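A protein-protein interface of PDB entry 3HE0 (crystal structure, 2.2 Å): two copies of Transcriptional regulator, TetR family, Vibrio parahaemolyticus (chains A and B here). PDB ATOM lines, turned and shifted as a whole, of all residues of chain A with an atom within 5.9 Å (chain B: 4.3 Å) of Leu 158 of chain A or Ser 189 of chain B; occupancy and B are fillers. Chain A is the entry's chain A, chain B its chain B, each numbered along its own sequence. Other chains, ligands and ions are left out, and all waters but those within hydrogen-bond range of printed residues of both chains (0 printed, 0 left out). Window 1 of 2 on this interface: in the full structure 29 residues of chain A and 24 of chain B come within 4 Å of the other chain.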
ATOM      1  N   LEU A 150      20.338  18.360  -0.587  1.00  0.00           N
ATOM      2  CA  LEU A 150      19.112  18.258  -1.356  1.00  0.00           C
ATOM      3  C   LEU A 150      18.025  18.774  -0.458  1.00  0.00           C
ATOM      4  O   LEU A 150      18.190  18.772   0.765  1.00  0.00           O
ATOM      5  CB  LEU A 150      18.873  16.790  -1.778  1.00  0.00           C
ATOM      6  CG  LEU A 150      19.957  16.165  -2.680  1.00  0.00           C
ATOM      7  CD1 LEU A 150      19.672  14.680  -2.973  1.00  0.00           C
ATOM      8  CD2 LEU A 150      20.135  16.932  -4.016  1.00  0.00           C
ATOM      9  N   GLU A 153      12.585  17.374   1.481  1.00  0.00           N
ATOM     10  CA  GLU A 153      11.576  16.523   0.845  1.00  0.00           C
ATOM     11  C   GLU A 153      12.202  15.405   0.010  1.00  0.00           C
ATOM     12  O   GLU A 153      11.666  14.281  -0.033  1.00  0.00           O
ATOM     13  CB  GLU A 153      10.635  17.352  -0.049  1.00  0.00           C
ATOM     14  CG  GLU A 153       9.574  18.145   0.738  1.00  0.00           C
ATOM     15  CD  GLU A 153       8.599  17.239   1.508  1.00  0.00           C
ATOM     16  OE1 GLU A 153       8.279  16.131   1.002  1.00  0.00           O
ATOM     17  OE2 GLU A 153       8.150  17.632   2.627  1.00  0.00           O
ATOM     18  N   VAL A 154      13.333  15.714  -0.633  1.00  0.00           N
ATOM     19  CA  VAL A 154      14.051  14.727  -1.449  1.00  0.00           C
ATOM     20  C   VAL A 154      14.793  13.762  -0.506  1.00  0.00           C
ATOM     21  O   VAL A 154      14.708  12.549  -0.638  1.00  0.00           O
ATOM     22  CB  VAL A 154      14.997  15.416  -2.425  1.00  0.00           C
ATOM     23  CG1 VAL A 154      15.867  14.392  -3.219  1.00  0.00           C
ATOM     24  CG2 VAL A 154      14.204  16.315  -3.372  1.00  0.00           C
ATOM     25  N   LEU A 155      15.486  14.302   0.490  1.00  0.00           N
ATOM     26  CA  LEU A 155      16.166  13.462   1.460  1.00  0.00           C
ATOM     27  C   LEU A 155      15.159  12.494   2.118  1.00  0.00           C
ATOM     28  O   LEU A 155      15.425  11.302   2.271  1.00  0.00           O
ATOM     29  CB  LEU A 155      16.870  14.331   2.505  1.00  0.00           C
ATOM     30  CG  LEU A 155      18.017  15.209   1.983  1.00  0.00           C
ATOM     31  CD1 LEU A 155      18.560  16.089   3.127  1.00  0.00           C
ATOM     32  CD2 LEU A 155      19.125  14.359   1.329  1.00  0.00           C
ATOM     33  N   SER A 156      13.969  12.997   2.452  1.00  0.00           N
ATOM     34  CA  SER A 156      12.957  12.141   3.071  1.00  0.00           C
ATOM     35  C   SER A 156      12.503  11.052   2.100  1.00  0.00           C
ATOM     36  O   SER A 156      12.436   9.877   2.472  1.00  0.00           O
ATOM     37  CB  SER A 156      11.763  12.948   3.574  1.00  0.00           C
ATOM     38  OG  SER A 156      10.850  12.104   4.315  1.00  0.00           O
ATOM     39  N   GLY A 157      12.243  11.443   0.854  1.00  0.00           N
ATOM     40  CA  GLY A 157      11.835  10.491  -0.179  1.00  0.00           C
ATOM     41  C   GLY A 157      12.861   9.388  -0.413  1.00  0.00           C
ATOM     42  O   GLY A 157      12.492   8.286  -0.728  1.00  0.00           O
ATOM     43  N   LEU A 158      14.148   9.690  -0.236  1.00  0.00           N
ATOM     44  CA  LEU A 158      15.219   8.738  -0.513  1.00  0.00           C
ATOM     45  C   LEU A 158      15.499   7.762   0.625  1.00  0.00           C
ATOM     46  O   LEU A 158      16.139   6.727   0.403  1.00  0.00           O
ATOM     47  CB  LEU A 158      16.504   9.495  -0.806  1.00  0.00           C
ATOM     48  CG  LEU A 158      16.576  10.225  -2.139  1.00  0.00           C
ATOM     49  CD1 LEU A 158      17.640  11.326  -1.969  1.00  0.00           C
ATOM     50  CD2 LEU A 158      16.802   9.268  -3.342  1.00  0.00           C
ATOM     51  N   SER A 159      14.997   8.072   1.822  1.00  0.00           N
ATOM     52  CA  SER A 159      15.381   7.365   3.021  1.00  0.00           C
ATOM     53  C   SER A 159      14.122   6.876   3.786  1.00  0.00           C
ATOM     54  O   SER A 159      13.608   5.778   3.512  1.00  0.00           O
ATOM     55  CB  SER A 159      16.297   8.253   3.872  1.00  0.00           C
ATOM     56  OG  SER A 159      15.662   9.450   4.276  1.00  0.00           O
ATOM     57  N   PHE A 160      13.584   7.707   4.668  1.00  0.00           N
ATOM     58  CA  PHE A 160      12.390   7.346   5.417  1.00  0.00           C
ATOM     59  C   PHE A 160      11.228   6.871   4.558  1.00  0.00           C
ATOM     60  O   PHE A 160      10.711   5.779   4.785  1.00  0.00           O
ATOM     61  CB  PHE A 160      11.931   8.518   6.290  1.00  0.00           C
ATOM     62  CG  PHE A 160      12.929   8.915   7.342  1.00  0.00           C
ATOM     63  CD1 PHE A 160      13.582   7.951   8.114  1.00  0.00           C
ATOM     64  CD2 PHE A 160      13.229  10.240   7.570  1.00  0.00           C
ATOM     65  CE1 PHE A 160      14.494   8.314   9.116  1.00  0.00           C
ATOM     66  CE2 PHE A 160      14.156  10.605   8.585  1.00  0.00           C
ATOM     67  CZ  PHE A 160      14.785   9.636   9.339  1.00  0.00           C
ATOM     68  N   GLU A 161      10.801   7.698   3.599  1.00  0.00           N
ATOM     69  CA  GLU A 161       9.533   7.465   2.867  1.00  0.00           C
ATOM     70  C   GLU A 161       9.638   6.210   2.045  1.00  0.00           C
ATOM     71  O   GLU A 161       8.626   5.519   1.791  1.00  0.00           O
ATOM     72  CB  GLU A 161       9.102   8.655   1.971  1.00  0.00           C
ATOM     73  CG  GLU A 161       8.388   9.794   2.767  1.00  0.00           C
ATOM     74  CD  GLU A 161       8.499  11.172   2.108  1.00  0.00           C
ATOM     75  OE1 GLU A 161       8.067  11.338   0.967  1.00  0.00           O
ATOM     76  OE2 GLU A 161       9.019  12.114   2.728  1.00  0.00           O
ATOM     77  N   ALA A 162      10.853   5.883   1.665  1.00  0.00           N
ATOM     78  CA  ALA A 162      11.040   4.711   0.832  1.00  0.00           C
ATOM     79  C   ALA A 162      10.875   3.471   1.696  1.00  0.00           C
ATOM     80  O   ALA A 162      10.204   2.526   1.285  1.00  0.00           O
ATOM     81  CB  ALA A 162      12.396   4.744   0.096  1.00  0.00           C
ATOM     82  N   SER A 189      19.978   2.762   3.336  1.00  0.00           N
ATOM     83  CA  SER A 189      19.188   3.981   3.201  1.00  0.00           C
ATOM     84  C   SER A 189      19.985   5.207   3.664  1.00  0.00           C
ATOM     85  O   SER A 189      19.876   6.265   3.060  1.00  0.00           O
ATOM     86  CB  SER A 189      17.822   3.847   3.902  1.00  0.00           C
ATOM     87  OG  SER A 189      17.922   3.686   5.296  1.00  0.00           O
ATOM     88  N   ALA A 192      22.020   6.494   0.937  1.00  0.00           N
ATOM     89  CA  ALA A 192      21.295   7.305  -0.035  1.00  0.00           C
ATOM     90  C   ALA A 192      21.435   8.789   0.315  1.00  0.00           C
ATOM     91  O   ALA A 192      21.565   9.594  -0.554  1.00  0.00           O
ATOM     92  CB  ALA A 192      19.807   6.900  -0.112  1.00  0.00           C
ATOM     93  N   ILE A 193      21.449   9.127   1.593  1.00  0.00           N
ATOM     94  CA  ILE A 193      21.390  10.532   2.001  1.00  0.00           C
ATOM     95  C   ILE A 193      22.734  11.139   2.394  1.00  0.00           C
ATOM     96  O   ILE A 193      22.870  12.375   2.401  1.00  0.00           O
ATOM     97  CB  ILE A 193      20.302  10.789   3.077  1.00  0.00           C
ATOM     98  CG1 ILE A 193      20.595   9.998   4.339  1.00  0.00           C
ATOM     99  CG2 ILE A 193      18.887  10.512   2.463  1.00  0.00           C
ATOM    100  CD1 ILE A 193      19.653  10.348   5.562  1.00  0.00           C
ATOM    101  N   TYR B  88      18.988   0.837 -14.922  1.00  0.00           N
ATOM    102  CA  TYR B  88      18.518   1.424 -13.690  1.00  0.00           C
ATOM    103  C   TYR B  88      17.871   2.765 -13.924  1.00  0.00           C
ATOM    104  O   TYR B  88      16.727   2.966 -13.508  1.00  0.00           O
ATOM    105  CB  TYR B  88      19.648   1.525 -12.655  1.00  0.00           C
ATOM    106  CG  TYR B  88      19.202   2.201 -11.391  1.00  0.00           C
ATOM    107  CD1 TYR B  88      18.534   1.494 -10.441  1.00  0.00           C
ATOM    108  CD2 TYR B  88      19.423   3.548 -11.167  1.00  0.00           C
ATOM    109  CE1 TYR B  88      18.116   2.067  -9.315  1.00  0.00           C
ATOM    110  CE2 TYR B  88      18.980   4.160  -9.984  1.00  0.00           C
ATOM    111  CZ  TYR B  88      18.332   3.405  -9.089  1.00  0.00           C
ATOM    112  OH  TYR B  88      17.867   3.926  -7.905  1.00  0.00           O
ATOM    113  N   TRP B  92      13.984   3.779 -13.374  1.00  0.00           N
ATOM    114  CA  TRP B  92      13.696   4.762 -12.341  1.00  0.00           C
ATOM    115  C   TRP B  92      12.797   5.854 -12.931  1.00  0.00           C
ATOM    116  O   TRP B  92      11.783   6.249 -12.326  1.00  0.00           O
ATOM    117  CB  TRP B  92      15.018   5.330 -11.821  1.00  0.00           C
ATOM    118  CG  TRP B  92      14.968   6.058 -10.503  1.00  0.00           C
ATOM    119  CD1 TRP B  92      15.390   5.572  -9.295  1.00  0.00           C
ATOM    120  CD2 TRP B  92      14.497   7.383 -10.259  1.00  0.00           C
ATOM    121  NE1 TRP B  92      15.191   6.516  -8.308  1.00  0.00           N
ATOM    122  CE2 TRP B  92      14.656   7.637  -8.878  1.00  0.00           C
ATOM    123  CE3 TRP B  92      13.957   8.382 -11.068  1.00  0.00           C
ATOM    124  CZ2 TRP B  92      14.304   8.839  -8.299  1.00  0.00           C
ATOM    125  CZ3 TRP B  92      13.609   9.591 -10.493  1.00  0.00           C
ATOM    126  CH2 TRP B  92      13.794   9.812  -9.112  1.00  0.00           C
ATOM    127  N   SER B 159      15.559   1.658  -3.532  1.00  0.00           N
ATOM    128  CA  SER B 159      15.880   2.443  -4.705  1.00  0.00           C
ATOM    129  C   SER B 159      14.630   2.871  -5.493  1.00  0.00           C
ATOM    130  O   SER B 159      14.188   4.003  -5.371  1.00  0.00           O
ATOM    131  CB  SER B 159      16.853   1.676  -5.594  1.00  0.00           C
ATOM    132  OG  SER B 159      16.371   0.402  -5.950  1.00  0.00           O
ATOM    133  N   ALA B 162      12.000   4.867  -3.875  1.00  0.00           N
ATOM    134  CA  ALA B 162      12.253   6.282  -3.714  1.00  0.00           C
ATOM    135  C   ALA B 162      11.686   6.979  -4.933  1.00  0.00           C
ATOM    136  O   ALA B 162      11.162   8.080  -4.818  1.00  0.00           O
ATOM    137  CB  ALA B 162      13.775   6.605  -3.540  1.00  0.00           C
ATOM    138  N   ALA B 185      18.753  12.999  -7.379  1.00  0.00           N
ATOM    139  CA  ALA B 185      17.963  11.991  -6.684  1.00  0.00           C
ATOM    140  C   ALA B 185      18.203  10.630  -7.314  1.00  0.00           C
ATOM    141  O   ALA B 185      18.273   9.635  -6.614  1.00  0.00           O
ATOM    142  CB  ALA B 185      16.476  12.329  -6.699  1.00  0.00           C
ATOM    143  N   ILE B 186      18.331  10.570  -8.636  1.00  0.00           N
ATOM    144  CA  ILE B 186      18.642   9.287  -9.257  1.00  0.00           C
ATOM    145  C   ILE B 186      19.994   8.806  -8.743  1.00  0.00           C
ATOM    146  O   ILE B 186      20.131   7.658  -8.364  1.00  0.00           O
ATOM    147  CB  ILE B 186      18.689   9.354 -10.778  1.00  0.00           C
ATOM    148  CG1 ILE B 186      17.289   9.657 -11.356  1.00  0.00           C
ATOM    149  CG2 ILE B 186      19.241   8.032 -11.321  1.00  0.00           C
ATOM    150  CD1 ILE B 186      17.260   9.854 -12.888  1.00  0.00           C
ATOM    151  N   GLU B 187      20.991   9.689  -8.662  1.00  0.00           N
ATOM    152  CA  GLU B 187      22.293   9.240  -8.124  1.00  0.00           C
ATOM    153  C   GLU B 187      22.223   8.817  -6.685  1.00  0.00           C
ATOM    154  O   GLU B 187      22.879   7.859  -6.301  1.00  0.00           O
ATOM    155  CB  GLU B 187      23.374  10.324  -8.188  1.00  0.00           C
ATOM    156  CG  GLU B 187      23.805  10.623  -9.546  1.00  0.00           C
ATOM    157  CD  GLU B 187      24.568   9.445 -10.211  1.00  0.00           C
ATOM    158  OE1 GLU B 187      25.048   8.514  -9.481  1.00  0.00           O
ATOM    159  OE2 GLU B 187      24.668   9.526 -11.479  1.00  0.00           O
ATOM    160  N   ALA B 188      21.503   9.582  -5.869  1.00  0.00           N
ATOM    161  CA  ALA B 188      21.393   9.254  -4.463  1.00  0.00           C
ATOM    162  C   ALA B 188      20.783   7.870  -4.252  1.00  0.00           C
ATOM    163  O   ALA B 188      21.261   7.079  -3.401  1.00  0.00           O
ATOM    164  CB  ALA B 188      20.587  10.349  -3.681  1.00  0.00           C
ATOM    165  N   SER B 189      19.727   7.543  -5.000  1.00  0.00           N
ATOM    166  CA  SER B 189      19.088   6.244  -4.799  1.00  0.00           C
ATOM    167  C   SER B 189      19.980   5.077  -5.305  1.00  0.00           C
ATOM    168  O   SER B 189      19.937   3.968  -4.755  1.00  0.00           O
ATOM    169  CB  SER B 189      17.689   6.213  -5.416  1.00  0.00           C
ATOM    170  OG  SER B 189      17.759   6.321  -6.802  1.00  0.00           O
ATOM    171  N   TRP B 190      20.830   5.347  -6.293  1.00  0.00           N
ATOM    172  CA  TRP B 190      21.867   4.417  -6.707  1.00  0.00           C
ATOM    173  C   TRP B 190      22.842   4.162  -5.566  1.00  0.00           C
ATOM    174  O   TRP B 190      23.215   3.030  -5.347  1.00  0.00           O
ATOM    175  CB  TRP B 190      22.607   4.955  -7.925  1.00  0.00           C
ATOM    176  CG  TRP B 190      23.705   4.133  -8.548  1.00  0.00           C
ATOM    177  CD1 TRP B 190      25.005   4.418  -8.510  1.00  0.00           C
ATOM    178  CD2 TRP B 190      23.573   2.985  -9.421  1.00  0.00           C
ATOM    179  NE1 TRP B 190      25.715   3.523  -9.266  1.00  0.00           N
ATOM    180  CE2 TRP B 190      24.860   2.617  -9.817  1.00  0.00           C
ATOM    181  CE3 TRP B 190      22.495   2.218  -9.868  1.00  0.00           C
ATOM    182  CZ2 TRP B 190      25.116   1.509 -10.672  1.00  0.00           C
ATOM    183  CZ3 TRP B 190      22.751   1.113 -10.731  1.00  0.00           C
ATOM    184  CH2 TRP B 190      24.034   0.771 -11.098  1.00  0.00           C
ATOM    185  N   ASP B 191      23.252   5.209  -4.857  1.00  0.00           N
ATOM    186  CA  ASP B 191      24.078   5.040  -3.679  1.00  0.00           C
ATOM    187  C   ASP B 191      23.475   4.062  -2.662  1.00  0.00           C
ATOM    188  O   ASP B 191      24.196   3.365  -1.952  1.00  0.00           O
ATOM    189  CB  ASP B 191      24.327   6.379  -2.971  1.00  0.00           C
ATOM    190  CG  ASP B 191      25.380   7.217  -3.648  1.00  0.00           C
ATOM    191  OD1 ASP B 191      26.108   6.696  -4.497  1.00  0.00           O
ATOM    192  OD2 ASP B 191      25.506   8.412  -3.315  1.00  0.00           O
ATOM    193  N   ALA B 192      22.154   4.022  -2.547  1.00  0.00           N
ATOM    194  CA  ALA B 192      21.554   3.138  -1.557  1.00  0.00           C
ATOM    195  C   ALA B 192      21.877   1.679  -1.883  1.00  0.00           C
ATOM    196  O   ALA B 192      22.057   0.890  -0.964  1.00  0.00           O
ATOM    197  CB  ALA B 192      20.034   3.331  -1.451  1.00  0.00           C
ATOM    198  N   ILE B 193      21.891   1.338  -3.174  1.00  0.00           N
ATOM    199  CA  ILE B 193      22.036  -0.057  -3.585  1.00  0.00           C
ATOM    200  C   ILE B 193      23.463  -0.505  -3.952  1.00  0.00           C
ATOM    201  O   ILE B 193      23.730  -1.692  -3.977  1.00  0.00           O
ATOM    202  CB  ILE B 193      21.042  -0.485  -4.711  1.00  0.00           C
ATOM    203  CG1 ILE B 193      21.196   0.364  -5.971  1.00  0.00           C
ATOM    204  CG2 ILE B 193      19.617  -0.493  -4.167  1.00  0.00           C
ATOM    205  CD1 ILE B 193      20.297  -0.124  -7.121  1.00  0.00           C
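Of chain B, only Ala 162, Ala 185, Ala 188 and Ser 189 come within 4 Å of Leu 158 of chain A. Ser 189 of chain B touches just one residue of chain A: Leu 158. Of the printed residues of chain B, Gly 157 of chain A touches Ala 162 (3.5 Å). Printed residues of chain A within 4 Å of Ala 185 of chain B: Leu 158. Of the printed residues of chain B, Ala 162 of chain A touches Ala 162 (3.99 Å). Of the printed residues of chain A, Ala 192 of chain B touches Ala 192 (3.8 Å). The nearest printed residue of chain B that does not touch Ala 162 of chain A is Ser 159 of chain B (5.7 Å).
Of the 14 printed residues of chain A, 4 touch a printed residue of chain B. Hydrophobic or aromatic side chains of chain A that line the printed part of chain B: Leu 158, Ala 162 and Ala 192. Hydrophobic or aromatic side chains of chain B within 4 Å of the printed part of chain A: Ala 162, Ala 188 and Ala 192. Among the printed residues, 8 pairs touch across the chains. Among the printed residues, no Asp or Glu carboxylate lies within 4 Å of a Lys or Arg side-chain nitrogen of the other chain.
Ala 162 of chain B touches Gly 157 of chain A. Ala 162 of chain B touches Leu 158 of chain A. O of Ala 185 of chain B touches CD2 of Leu 158 of chain A, 3.6 Å away. CD1 of Leu 158 of chain A touches CB of Ala 188 of chain B, 3.5 Å away. CD2 of Leu 158 of chain A touches N of Ser 189 of chain B, at 3.8 Å. Ala 162 of chain A touches Ala 162 of chain B. Ala 192 of chain A touches Ala 188 of chain B (O to CB, 3.4 Å). Ala 192 of chain A touches Ala 192 of chain B.
Ala 162 of chain B touches its own counterpart, Ala 162 of chain A. Ala 192 of chain B touches its own counterpart, Ala 192 of chain A. Positions printed for both chains: 159, 162, 189, 192 and 193. Of the 8 pairs that touch across the chains among the printed residues, 2 have their exchanged pair printed and touching as well.
The backbone carbonyl oxygen (O) of Ile 186 of chain B sits at hydrogen-bond distance from the side-chain hydroxyl (OG) of Ser 189 of chain B, at 3.1 Å. The side-chain hydroxyl of Tyr 88 of chain B is in hydrogen-bond range of the side-chain hydroxyl of Ser 189 of chain B. OG of Ser 189 of chain B is in hydrogen-bond range of O of Ala 185 of chain B. The indole nitrogen (NE1) of Trp 92 of chain B sits at hydrogen-bond distance from the side-chain hydroxyl (OG) of Ser 189 of chain B (3.0 Å).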
